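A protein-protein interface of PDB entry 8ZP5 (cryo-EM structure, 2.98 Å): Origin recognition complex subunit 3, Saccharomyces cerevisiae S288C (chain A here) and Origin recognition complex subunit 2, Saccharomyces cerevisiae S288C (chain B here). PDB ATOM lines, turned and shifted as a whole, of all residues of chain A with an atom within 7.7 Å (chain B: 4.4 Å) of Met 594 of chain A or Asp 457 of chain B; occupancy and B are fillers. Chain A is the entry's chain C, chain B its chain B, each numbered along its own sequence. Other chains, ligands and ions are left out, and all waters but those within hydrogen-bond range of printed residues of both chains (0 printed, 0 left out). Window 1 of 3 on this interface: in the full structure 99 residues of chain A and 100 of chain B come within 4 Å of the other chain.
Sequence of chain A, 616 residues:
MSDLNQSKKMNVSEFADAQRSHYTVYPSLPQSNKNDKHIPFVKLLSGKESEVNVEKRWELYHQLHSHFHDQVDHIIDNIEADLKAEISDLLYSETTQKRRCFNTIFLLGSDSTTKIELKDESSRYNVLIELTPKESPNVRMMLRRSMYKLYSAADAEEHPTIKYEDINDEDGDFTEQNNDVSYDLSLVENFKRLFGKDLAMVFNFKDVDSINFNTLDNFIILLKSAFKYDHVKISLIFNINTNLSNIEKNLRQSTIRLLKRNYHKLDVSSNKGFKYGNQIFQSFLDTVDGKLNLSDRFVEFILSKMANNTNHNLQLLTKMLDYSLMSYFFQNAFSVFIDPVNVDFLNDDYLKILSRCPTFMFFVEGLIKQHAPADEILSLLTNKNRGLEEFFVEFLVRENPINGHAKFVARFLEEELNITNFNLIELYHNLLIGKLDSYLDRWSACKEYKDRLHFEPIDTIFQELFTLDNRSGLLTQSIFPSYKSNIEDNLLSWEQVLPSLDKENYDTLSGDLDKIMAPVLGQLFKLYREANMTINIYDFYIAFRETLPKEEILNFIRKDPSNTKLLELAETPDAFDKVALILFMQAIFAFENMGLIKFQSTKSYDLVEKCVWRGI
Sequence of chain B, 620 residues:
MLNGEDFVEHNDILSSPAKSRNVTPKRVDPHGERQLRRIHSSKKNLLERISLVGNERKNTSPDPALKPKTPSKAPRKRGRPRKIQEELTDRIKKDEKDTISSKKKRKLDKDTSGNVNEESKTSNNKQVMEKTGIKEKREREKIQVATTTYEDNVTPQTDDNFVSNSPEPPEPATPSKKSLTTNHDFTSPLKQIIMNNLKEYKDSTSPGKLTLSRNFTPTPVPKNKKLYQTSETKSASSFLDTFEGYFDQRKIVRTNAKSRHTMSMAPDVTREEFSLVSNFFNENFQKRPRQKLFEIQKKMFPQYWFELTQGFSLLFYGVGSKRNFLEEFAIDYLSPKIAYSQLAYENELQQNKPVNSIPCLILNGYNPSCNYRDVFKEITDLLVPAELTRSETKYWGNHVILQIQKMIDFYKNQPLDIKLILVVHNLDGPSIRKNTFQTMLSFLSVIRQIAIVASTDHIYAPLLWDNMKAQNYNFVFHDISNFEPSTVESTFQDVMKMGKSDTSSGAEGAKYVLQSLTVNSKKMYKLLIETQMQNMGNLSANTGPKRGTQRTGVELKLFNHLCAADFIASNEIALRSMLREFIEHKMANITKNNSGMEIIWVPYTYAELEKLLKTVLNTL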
ATOM      1  N   TYR A 483     -14.618  16.133  -0.229  1.00  0.00           N
ATOM      2  CA  TYR A 483     -15.280  17.143   0.591  1.00  0.00           C
ATOM      3  C   TYR A 483     -14.908  18.551   0.141  1.00  0.00           C
ATOM      4  O   TYR A 483     -15.765  19.335  -0.294  1.00  0.00           O
ATOM      5  CB  TYR A 483     -14.897  16.920   2.055  1.00  0.00           C
ATOM      6  CG  TYR A 483     -15.805  17.559   3.079  1.00  0.00           C
ATOM      7  CD1 TYR A 483     -15.686  18.904   3.396  1.00  0.00           C
ATOM      8  CD2 TYR A 483     -16.760  16.810   3.748  1.00  0.00           C
ATOM      9  CE1 TYR A 483     -16.505  19.487   4.339  1.00  0.00           C
ATOM     10  CE2 TYR A 483     -17.583  17.386   4.693  1.00  0.00           C
ATOM     11  CZ  TYR A 483     -17.451  18.725   4.982  1.00  0.00           C
ATOM     12  OH  TYR A 483     -18.267  19.308   5.921  1.00  0.00           O
ATOM     13  N   ILE A 487     -17.228  21.154  -2.152  1.00  0.00           N
ATOM     14  CA  ILE A 487     -17.660  22.446  -1.622  1.00  0.00           C
ATOM     15  C   ILE A 487     -17.148  23.585  -2.497  1.00  0.00           C
ATOM     16  O   ILE A 487     -17.881  24.535  -2.800  1.00  0.00           O
ATOM     17  CB  ILE A 487     -17.212  22.606  -0.158  1.00  0.00           C
ATOM     18  CG1 ILE A 487     -17.966  21.621   0.736  1.00  0.00           C
ATOM     19  CG2 ILE A 487     -17.437  24.032   0.318  1.00  0.00           C
ATOM     20  CD1 ILE A 487     -17.822  21.904   2.210  1.00  0.00           C
ATOM     21  N   LEU A 491     -19.244  26.338  -4.661  1.00  0.00           N
ATOM     22  CA  LEU A 491     -19.055  27.777  -4.504  1.00  0.00           C
ATOM     23  C   LEU A 491     -18.738  28.443  -5.837  1.00  0.00           C
ATOM     24  O   LEU A 491     -19.381  29.426  -6.220  1.00  0.00           O
ATOM     25  CB  LEU A 491     -17.940  28.050  -3.496  1.00  0.00           C
ATOM     26  CG  LEU A 491     -18.312  28.010  -2.016  1.00  0.00           C
ATOM     27  CD1 LEU A 491     -17.062  27.945  -1.157  1.00  0.00           C
ATOM     28  CD2 LEU A 491     -19.151  29.219  -1.652  1.00  0.00           C
ATOM     29  N   LEU A 521     -22.356  34.283  -2.067  1.00  0.00           N
ATOM     30  CA  LEU A 521     -21.274  33.371  -1.713  1.00  0.00           C
ATOM     31  C   LEU A 521     -20.464  32.969  -2.940  1.00  0.00           C
ATOM     32  O   LEU A 521     -19.230  32.995  -2.916  1.00  0.00           O
ATOM     33  CB  LEU A 521     -21.839  32.135  -1.013  1.00  0.00           C
ATOM     34  CG  LEU A 521     -22.172  32.283   0.470  1.00  0.00           C
ATOM     35  CD1 LEU A 521     -23.315  31.361   0.854  1.00  0.00           C
ATOM     36  CD2 LEU A 521     -20.948  31.996   1.313  1.00  0.00           C
ATOM     37  N   PHE A 525     -16.705  34.071  -3.786  1.00  0.00           N
ATOM     38  CA  PHE A 525     -15.672  33.049  -3.917  1.00  0.00           C
ATOM     39  C   PHE A 525     -14.926  33.170  -5.237  1.00  0.00           C
ATOM     40  O   PHE A 525     -13.737  32.850  -5.303  1.00  0.00           O
ATOM     41  CB  PHE A 525     -16.265  31.650  -3.786  1.00  0.00           C
ATOM     42  CG  PHE A 525     -15.245  30.553  -3.916  1.00  0.00           C
ATOM     43  CD1 PHE A 525     -14.446  30.205  -2.843  1.00  0.00           C
ATOM     44  CD2 PHE A 525     -15.073  29.884  -5.116  1.00  0.00           C
ATOM     45  CE1 PHE A 525     -13.502  29.205  -2.960  1.00  0.00           C
ATOM     46  CE2 PHE A 525     -14.133  28.884  -5.238  1.00  0.00           C
ATOM     47  CZ  PHE A 525     -13.346  28.544  -4.159  1.00  0.00           C
ATOM     48  N   ALA A 587     -21.228  37.652   3.584  1.00  0.00           N
ATOM     49  CA  ALA A 587     -20.483  36.622   2.866  1.00  0.00           C
ATOM     50  C   ALA A 587     -19.120  36.364   3.503  1.00  0.00           C
ATOM     51  O   ALA A 587     -18.662  35.217   3.553  1.00  0.00           O
ATOM     52  CB  ALA A 587     -20.332  37.019   1.401  1.00  0.00           C
ATOM     53  N   ILE A 588     -18.449  37.416   3.980  1.00  0.00           N
ATOM     54  CA  ILE A 588     -17.173  37.237   4.667  1.00  0.00           C
ATOM     55  C   ILE A 588     -17.368  36.464   5.963  1.00  0.00           C
ATOM     56  O   ILE A 588     -16.551  35.606   6.319  1.00  0.00           O
ATOM     57  CB  ILE A 588     -16.500  38.599   4.913  1.00  0.00           C
ATOM     58  CG1 ILE A 588     -16.025  39.200   3.592  1.00  0.00           C
ATOM     59  CG2 ILE A 588     -15.336  38.464   5.880  1.00  0.00           C
ATOM     60  CD1 ILE A 588     -14.939  38.396   2.916  1.00  0.00           C
ATOM     61  N   PHE A 589     -18.448  36.754   6.690  1.00  0.00           N
ATOM     62  CA  PHE A 589     -18.758  35.980   7.886  1.00  0.00           C
ATOM     63  C   PHE A 589     -18.972  34.513   7.539  1.00  0.00           C
ATOM     64  O   PHE A 589     -18.493  33.621   8.251  1.00  0.00           O
ATOM     65  CB  PHE A 589     -19.989  36.579   8.576  1.00  0.00           C
ATOM     66  CG  PHE A 589     -20.459  35.814   9.785  1.00  0.00           C
ATOM     67  CD1 PHE A 589     -20.199  36.293  11.056  1.00  0.00           C
ATOM     68  CD2 PHE A 589     -21.210  34.656   9.654  1.00  0.00           C
ATOM     69  CE1 PHE A 589     -20.636  35.610  12.170  1.00  0.00           C
ATOM     70  CE2 PHE A 589     -21.648  33.969  10.765  1.00  0.00           C
ATOM     71  CZ  PHE A 589     -21.365  34.448  12.023  1.00  0.00           C
ATOM     72  N   ALA A 590     -19.681  34.244   6.442  1.00  0.00           N
ATOM     73  CA  ALA A 590     -19.900  32.861   6.025  1.00  0.00           C
ATOM     74  C   ALA A 590     -18.582  32.169   5.689  1.00  0.00           C
ATOM     75  O   ALA A 590     -18.335  31.038   6.122  1.00  0.00           O
ATOM     76  CB  ALA A 590     -20.854  32.819   4.833  1.00  0.00           C
ATOM     77  N   PHE A 591     -17.715  32.842   4.927  1.00  0.00           N
ATOM     78  CA  PHE A 591     -16.428  32.248   4.571  1.00  0.00           C
ATOM     79  C   PHE A 591     -15.573  31.989   5.804  1.00  0.00           C
ATOM     80  O   PHE A 591     -14.879  30.970   5.881  1.00  0.00           O
ATOM     81  CB  PHE A 591     -15.675  33.135   3.580  1.00  0.00           C
ATOM     82  CG  PHE A 591     -16.196  33.059   2.177  1.00  0.00           C
ATOM     83  CD1 PHE A 591     -17.055  32.043   1.798  1.00  0.00           C
ATOM     84  CD2 PHE A 591     -15.805  33.985   1.228  1.00  0.00           C
ATOM     85  CE1 PHE A 591     -17.528  31.964   0.505  1.00  0.00           C
ATOM     86  CE2 PHE A 591     -16.275  33.908  -0.066  1.00  0.00           C
ATOM     87  CZ  PHE A 591     -17.138  32.898  -0.427  1.00  0.00           C
ATOM     88  N   GLU A 592     -15.598  32.904   6.772  1.00  0.00           N
ATOM     89  CA  GLU A 592     -14.862  32.672   8.011  1.00  0.00           C
ATOM     90  C   GLU A 592     -15.435  31.482   8.769  1.00  0.00           C
ATOM     91  O   GLU A 592     -14.689  30.710   9.383  1.00  0.00           O
ATOM     92  CB  GLU A 592     -14.880  33.930   8.876  1.00  0.00           C
ATOM     93  CG  GLU A 592     -14.165  33.778  10.206  1.00  0.00           C
ATOM     94  CD  GLU A 592     -13.897  35.111  10.875  1.00  0.00           C
ATOM     95  OE1 GLU A 592     -13.595  36.086  10.155  1.00  0.00           O
ATOM     96  OE2 GLU A 592     -13.986  35.183  12.118  1.00  0.00           O
ATOM     97  N   ASN A 593     -16.760  31.318   8.739  1.00  0.00           N
ATOM     98  CA  ASN A 593     -17.375  30.162   9.387  1.00  0.00           C
ATOM     99  C   ASN A 593     -16.943  28.856   8.728  1.00  0.00           C
ATOM    100  O   ASN A 593     -16.646  27.876   9.420  1.00  0.00           O
ATOM    101  CB  ASN A 593     -18.897  30.291   9.366  1.00  0.00           C
ATOM    102  CG  ASN A 593     -19.451  30.826  10.669  1.00  0.00           C
ATOM    103  OD1 ASN A 593     -18.700  31.170  11.581  1.00  0.00           O
ATOM    104  ND2 ASN A 593     -20.773  30.888  10.768  1.00  0.00           N
ATOM    105  N   MET A 594     -16.904  28.819   7.396  1.00  0.00           N
ATOM    106  CA  MET A 594     -16.492  27.607   6.693  1.00  0.00           C
ATOM    107  C   MET A 594     -14.980  27.470   6.565  1.00  0.00           C
ATOM    108  O   MET A 594     -14.520  26.609   5.811  1.00  0.00           O
ATOM    109  CB  MET A 594     -17.132  27.539   5.303  1.00  0.00           C
ATOM    110  CG  MET A 594     -18.523  28.129   5.216  1.00  0.00           C
ATOM    111  SD  MET A 594     -19.304  27.864   3.613  1.00  0.00           S
ATOM    112  CE  MET A 594     -18.110  28.625   2.520  1.00  0.00           C
ATOM    113  N   GLY A 595     -14.202  28.288   7.268  1.00  0.00           N
ATOM    114  CA  GLY A 595     -12.761  28.127   7.261  1.00  0.00           C
ATOM    115  C   GLY A 595     -12.077  28.487   5.963  1.00  0.00           C
ATOM    116  O   GLY A 595     -10.977  27.997   5.698  1.00  0.00           O
ATOM    117  N   LEU A 596     -12.701  29.328   5.137  1.00  0.00           N
ATOM    118  CA  LEU A 596     -12.090  29.724   3.872  1.00  0.00           C
ATOM    119  C   LEU A 596     -10.997  30.767   4.072  1.00  0.00           C
ATOM    120  O   LEU A 596     -10.003  30.773   3.338  1.00  0.00           O
ATOM    121  CB  LEU A 596     -13.160  30.250   2.913  1.00  0.00           C
ATOM    122  CG  LEU A 596     -13.863  29.259   1.981  1.00  0.00           C
ATOM    123  CD1 LEU A 596     -12.894  28.712   0.954  1.00  0.00           C
ATOM    124  CD2 LEU A 596     -14.506  28.123   2.754  1.00  0.00           C
ATOM    125  N   ILE A 597     -11.160  31.657   5.053  1.00  0.00           N
ATOM    126  CA  ILE A 597     -10.228  32.753   5.282  1.00  0.00           C
ATOM    127  C   ILE A 597      -9.795  32.747   6.740  1.00  0.00           C
ATOM    128  O   ILE A 597     -10.445  32.156   7.606  1.00  0.00           O
ATOM    129  CB  ILE A 597     -10.838  34.126   4.923  1.00  0.00           C
ATOM    130  CG1 ILE A 597     -11.843  34.558   5.991  1.00  0.00           C
ATOM    131  CG2 ILE A 597     -11.519  34.082   3.574  1.00  0.00           C
ATOM    132  CD1 ILE A 597     -12.482  35.895   5.718  1.00  0.00           C
ATOM    133  N   CYS A 611      -7.166  30.447   3.158  1.00  0.00           N
ATOM    134  CA  CYS A 611      -6.839  29.157   3.742  1.00  0.00           C
ATOM    135  C   CYS A 611      -7.155  27.986   2.827  1.00  0.00           C
ATOM    136  O   CYS A 611      -6.694  26.872   3.095  1.00  0.00           O
ATOM    137  CB  CYS A 611      -7.583  28.968   5.072  1.00  0.00           C
ATOM    138  SG  CYS A 611      -6.989  30.014   6.415  1.00  0.00           S
ATOM    139  N   VAL A 612      -7.923  28.202   1.763  1.00  0.00           N
ATOM    140  CA  VAL A 612      -8.341  27.136   0.862  1.00  0.00           C
ATOM    141  C   VAL A 612      -8.060  27.571  -0.568  1.00  0.00           C
ATOM    142  O   VAL A 612      -8.509  28.641  -0.996  1.00  0.00           O
ATOM    143  CB  VAL A 612      -9.829  26.792   1.033  1.00  0.00           C
ATOM    144  CG1 VAL A 612     -10.246  25.761   0.008  1.00  0.00           C
ATOM    145  CG2 VAL A 612     -10.099  26.282   2.438  1.00  0.00           C
ATOM    146  N   VAL B 319     -22.763  24.248   1.071  1.00  0.00           N
ATOM    147  CA  VAL B 319     -22.731  25.684   1.320  1.00  0.00           C
ATOM    148  C   VAL B 319     -24.158  26.152   1.575  1.00  0.00           C
ATOM    149  O   VAL B 319     -25.052  25.938   0.748  1.00  0.00           O
ATOM    150  CB  VAL B 319     -22.076  26.448   0.159  1.00  0.00           C
ATOM    151  CG1 VAL B 319     -20.598  26.128   0.105  1.00  0.00           C
ATOM    152  CG2 VAL B 319     -22.719  26.079  -1.166  1.00  0.00           C
ATOM    153  N   GLY B 320     -24.375  26.767   2.731  1.00  0.00           N
ATOM    154  CA  GLY B 320     -25.676  27.248   3.133  1.00  0.00           C
ATOM    155  C   GLY B 320     -26.092  26.642   4.450  1.00  0.00           C
ATOM    156  O   GLY B 320     -25.333  25.919   5.102  1.00  0.00           O
ATOM    157  N   LYS B 322     -28.087  24.063   6.427  1.00  0.00           N
ATOM    158  CA  LYS B 322     -28.749  22.769   6.381  1.00  0.00           C
ATOM    159  C   LYS B 322     -29.632  22.527   7.597  1.00  0.00           C
ATOM    160  O   LYS B 322     -30.175  21.428   7.744  1.00  0.00           O
ATOM    161  CB  LYS B 322     -27.714  21.651   6.253  1.00  0.00           C
ATOM    162  CG  LYS B 322     -26.810  21.787   5.041  1.00  0.00           C
ATOM    163  CD  LYS B 322     -25.564  20.943   5.193  1.00  0.00           C
ATOM    164  CE  LYS B 322     -24.594  21.570   6.172  1.00  0.00           C
ATOM    165  NZ  LYS B 322     -23.939  22.774   5.597  1.00  0.00           N
ATOM    166  N   ASN B 426     -24.572  21.319  12.657  1.00  0.00           N
ATOM    167  CA  ASN B 426     -23.247  21.938  12.641  1.00  0.00           C
ATOM    168  C   ASN B 426     -22.287  21.208  13.586  1.00  0.00           C
ATOM    169  O   ASN B 426     -21.844  21.733  14.606  1.00  0.00           O
ATOM    170  CB  ASN B 426     -23.345  23.425  12.991  1.00  0.00           C
ATOM    171  CG  ASN B 426     -22.257  24.247  12.338  1.00  0.00           C
ATOM    172  OD1 ASN B 426     -21.423  23.720  11.603  1.00  0.00           O
ATOM    173  ND2 ASN B 426     -22.260  25.549  12.601  1.00  0.00           N
ATOM    174  N   ASP B 428     -19.312  20.606  13.452  1.00  0.00           N
ATOM    175  CA  ASP B 428     -17.984  21.188  13.585  1.00  0.00           C
ATOM    176  C   ASP B 428     -18.000  22.531  14.309  1.00  0.00           C
ATOM    177  O   ASP B 428     -17.043  23.304  14.186  1.00  0.00           O
ATOM    178  CB  ASP B 428     -17.339  21.347  12.210  1.00  0.00           C
ATOM    179  CG  ASP B 428     -18.201  22.142  11.254  1.00  0.00           C
ATOM    180  OD1 ASP B 428     -18.406  23.350  11.490  1.00  0.00           O
ATOM    181  OD2 ASP B 428     -18.673  21.560  10.259  1.00  0.00           O
ATOM    182  N   THR B 456     -22.336  19.276   8.695  1.00  0.00           N
ATOM    183  CA  THR B 456     -21.074  19.977   8.891  1.00  0.00           C
ATOM    184  C   THR B 456     -20.960  21.136   7.914  1.00  0.00           C
ATOM    185  O   THR B 456     -21.376  21.029   6.757  1.00  0.00           O
ATOM    186  CB  THR B 456     -19.868  19.044   8.716  1.00  0.00           C
ATOM    187  OG1 THR B 456     -19.884  18.477   7.400  1.00  0.00           O
ATOM    188  CG2 THR B 456     -19.881  17.941   9.756  1.00  0.00           C
ATOM    189  N   ASP B 457     -20.386  22.241   8.388  1.00  0.00           N
ATOM    190  CA  ASP B 457     -20.165  23.427   7.573  1.00  0.00           C
ATOM    191  C   ASP B 457     -18.700  23.714   7.290  1.00  0.00           C
ATOM    192  O   ASP B 457     -18.385  24.235   6.219  1.00  0.00           O
ATOM    193  CB  ASP B 457     -20.786  24.660   8.242  1.00  0.00           C
ATOM    194  CG  ASP B 457     -22.299  24.624   8.240  1.00  0.00           C
ATOM    195  OD1 ASP B 457     -22.879  24.024   7.312  1.00  0.00           O
ATOM    196  OD2 ASP B 457     -22.912  25.197   9.164  1.00  0.00           O
ATOM    197  N   HIS B 458     -17.803  23.392   8.219  1.00  0.00           N
ATOM    198  CA  HIS B 458     -16.387  23.664   8.019  1.00  0.00           C
ATOM    199  C   HIS B 458     -15.842  22.839   6.860  1.00  0.00           C
ATOM    200  O   HIS B 458     -16.271  21.710   6.614  1.00  0.00           O
ATOM    201  CB  HIS B 458     -15.599  23.363   9.293  1.00  0.00           C
ATOM    202  CG  HIS B 458     -14.317  24.127   9.404  1.00  0.00           C
ATOM    203  ND1 HIS B 458     -13.126  23.662   8.889  1.00  0.00           N
ATOM    204  CD2 HIS B 458     -14.039  25.324   9.972  1.00  0.00           C
ATOM    205  CE1 HIS B 458     -12.170  24.541   9.135  1.00  0.00           C
ATOM    206  NE2 HIS B 458     -12.698  25.557   9.792  1.00  0.00           N
ATOM    207  N   ILE B 459     -14.880  23.421   6.142  1.00  0.00           N
ATOM    208  CA  ILE B 459     -14.333  22.761   4.962  1.00  0.00           C
ATOM    209  C   ILE B 459     -13.272  21.731   5.331  1.00  0.00           C
ATOM    210  O   ILE B 459     -13.008  20.813   4.546  1.00  0.00           O
ATOM    211  CB  ILE B 459     -13.773  23.812   3.989  1.00  0.00           C
ATOM    212  CG1 ILE B 459     -13.483  23.193   2.626  1.00  0.00           C
ATOM    213  CG2 ILE B 459     -12.506  24.433   4.546  1.00  0.00           C
ATOM    214  CD1 ILE B 459     -13.248  24.208   1.538  1.00  0.00           C
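OH of Tyr 483 of chain A lies close to OG1 of Thr 456 of chain B, 2.3 Å away.
O of Met 594 of chain A lies close to N of Ile 459 of chain B (3.2 Å).
O of His 458 of chain B sits close to OH of Tyr 483 of chain A, at 3.2 Å.
The side-chain carboxylate of Asp 428 of chain B is in hydrogen-bond range of the backbone NH of Asp 457 of chain B, at 2.6 Å.
OD1 of Asn 426 of chain B lies close to OD2 of Asp 457 of chain B (3.2 Å).
The backbone NH (N) of His 458 of chain B is in hydrogen-bond range of the side-chain carboxylate (OD2) of Asp 428 of chain B, 2.9 Å away.
The backbone carbonyl oxygen (O) of Thr 456 of chain B is in hydrogen-bond range of the side-chain amino group (NZ) of Lys 322 of chain B (3.3 Å).
Ile 459 of chain B touches Tyr 483 of chain A (O to CD1, 3.5 Å).
Ile 487 of chain A touches Val 319 of chain B.
CG of Leu 491 of chain A touches CG1 of Val 319 of chain B, at 3.6 Å.
His 458 of chain B touches Asn 593 of chain A (CD2 to O, 3.7 Å).
Asp 457 of chain B touches Met 594 of chain A (O to CB, 3.7 Å).
Gly 595 of chain A touches His 458 of chain B.
Ile 459 of chain B touches Val 612 of chain A (CG2 to CG2, 3.7 Å).
Printed residues of chain B within 4 Å of Tyr 483 of chain A: Thr 456, His 458 and Ile 459.
Phe 589 of chain A touches none of the printed residues of chain B.
Of chain B, only Asp 457 (3.7 Å) and Ile 459 (3.2 Å) come within 4 Å of Met 594 of chain A.
Asp 457 of chain B touches just one residue of chain A: Met 594 (3.7 Å).
Printed residues of chain A within 4 Å of Ile 459 of chain B: Tyr 483 (3.5 Å), Met 594 (3.2 Å) and Val 612 (3.7 Å).
The nearest printed residue of chain B that does not touch Val 612 of chain A is His 458 of chain B (7.2 Å).
Hydrophobic or aromatic side chains of chain A that line the printed part of chain B: Tyr 483, Ile 487, Leu 491, Met 594 and Val 612.
Of the 9 printed residues of chain B, 5 touch a printed residue of chain A.
Among the printed residues, 10 pairs touch across the chains.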
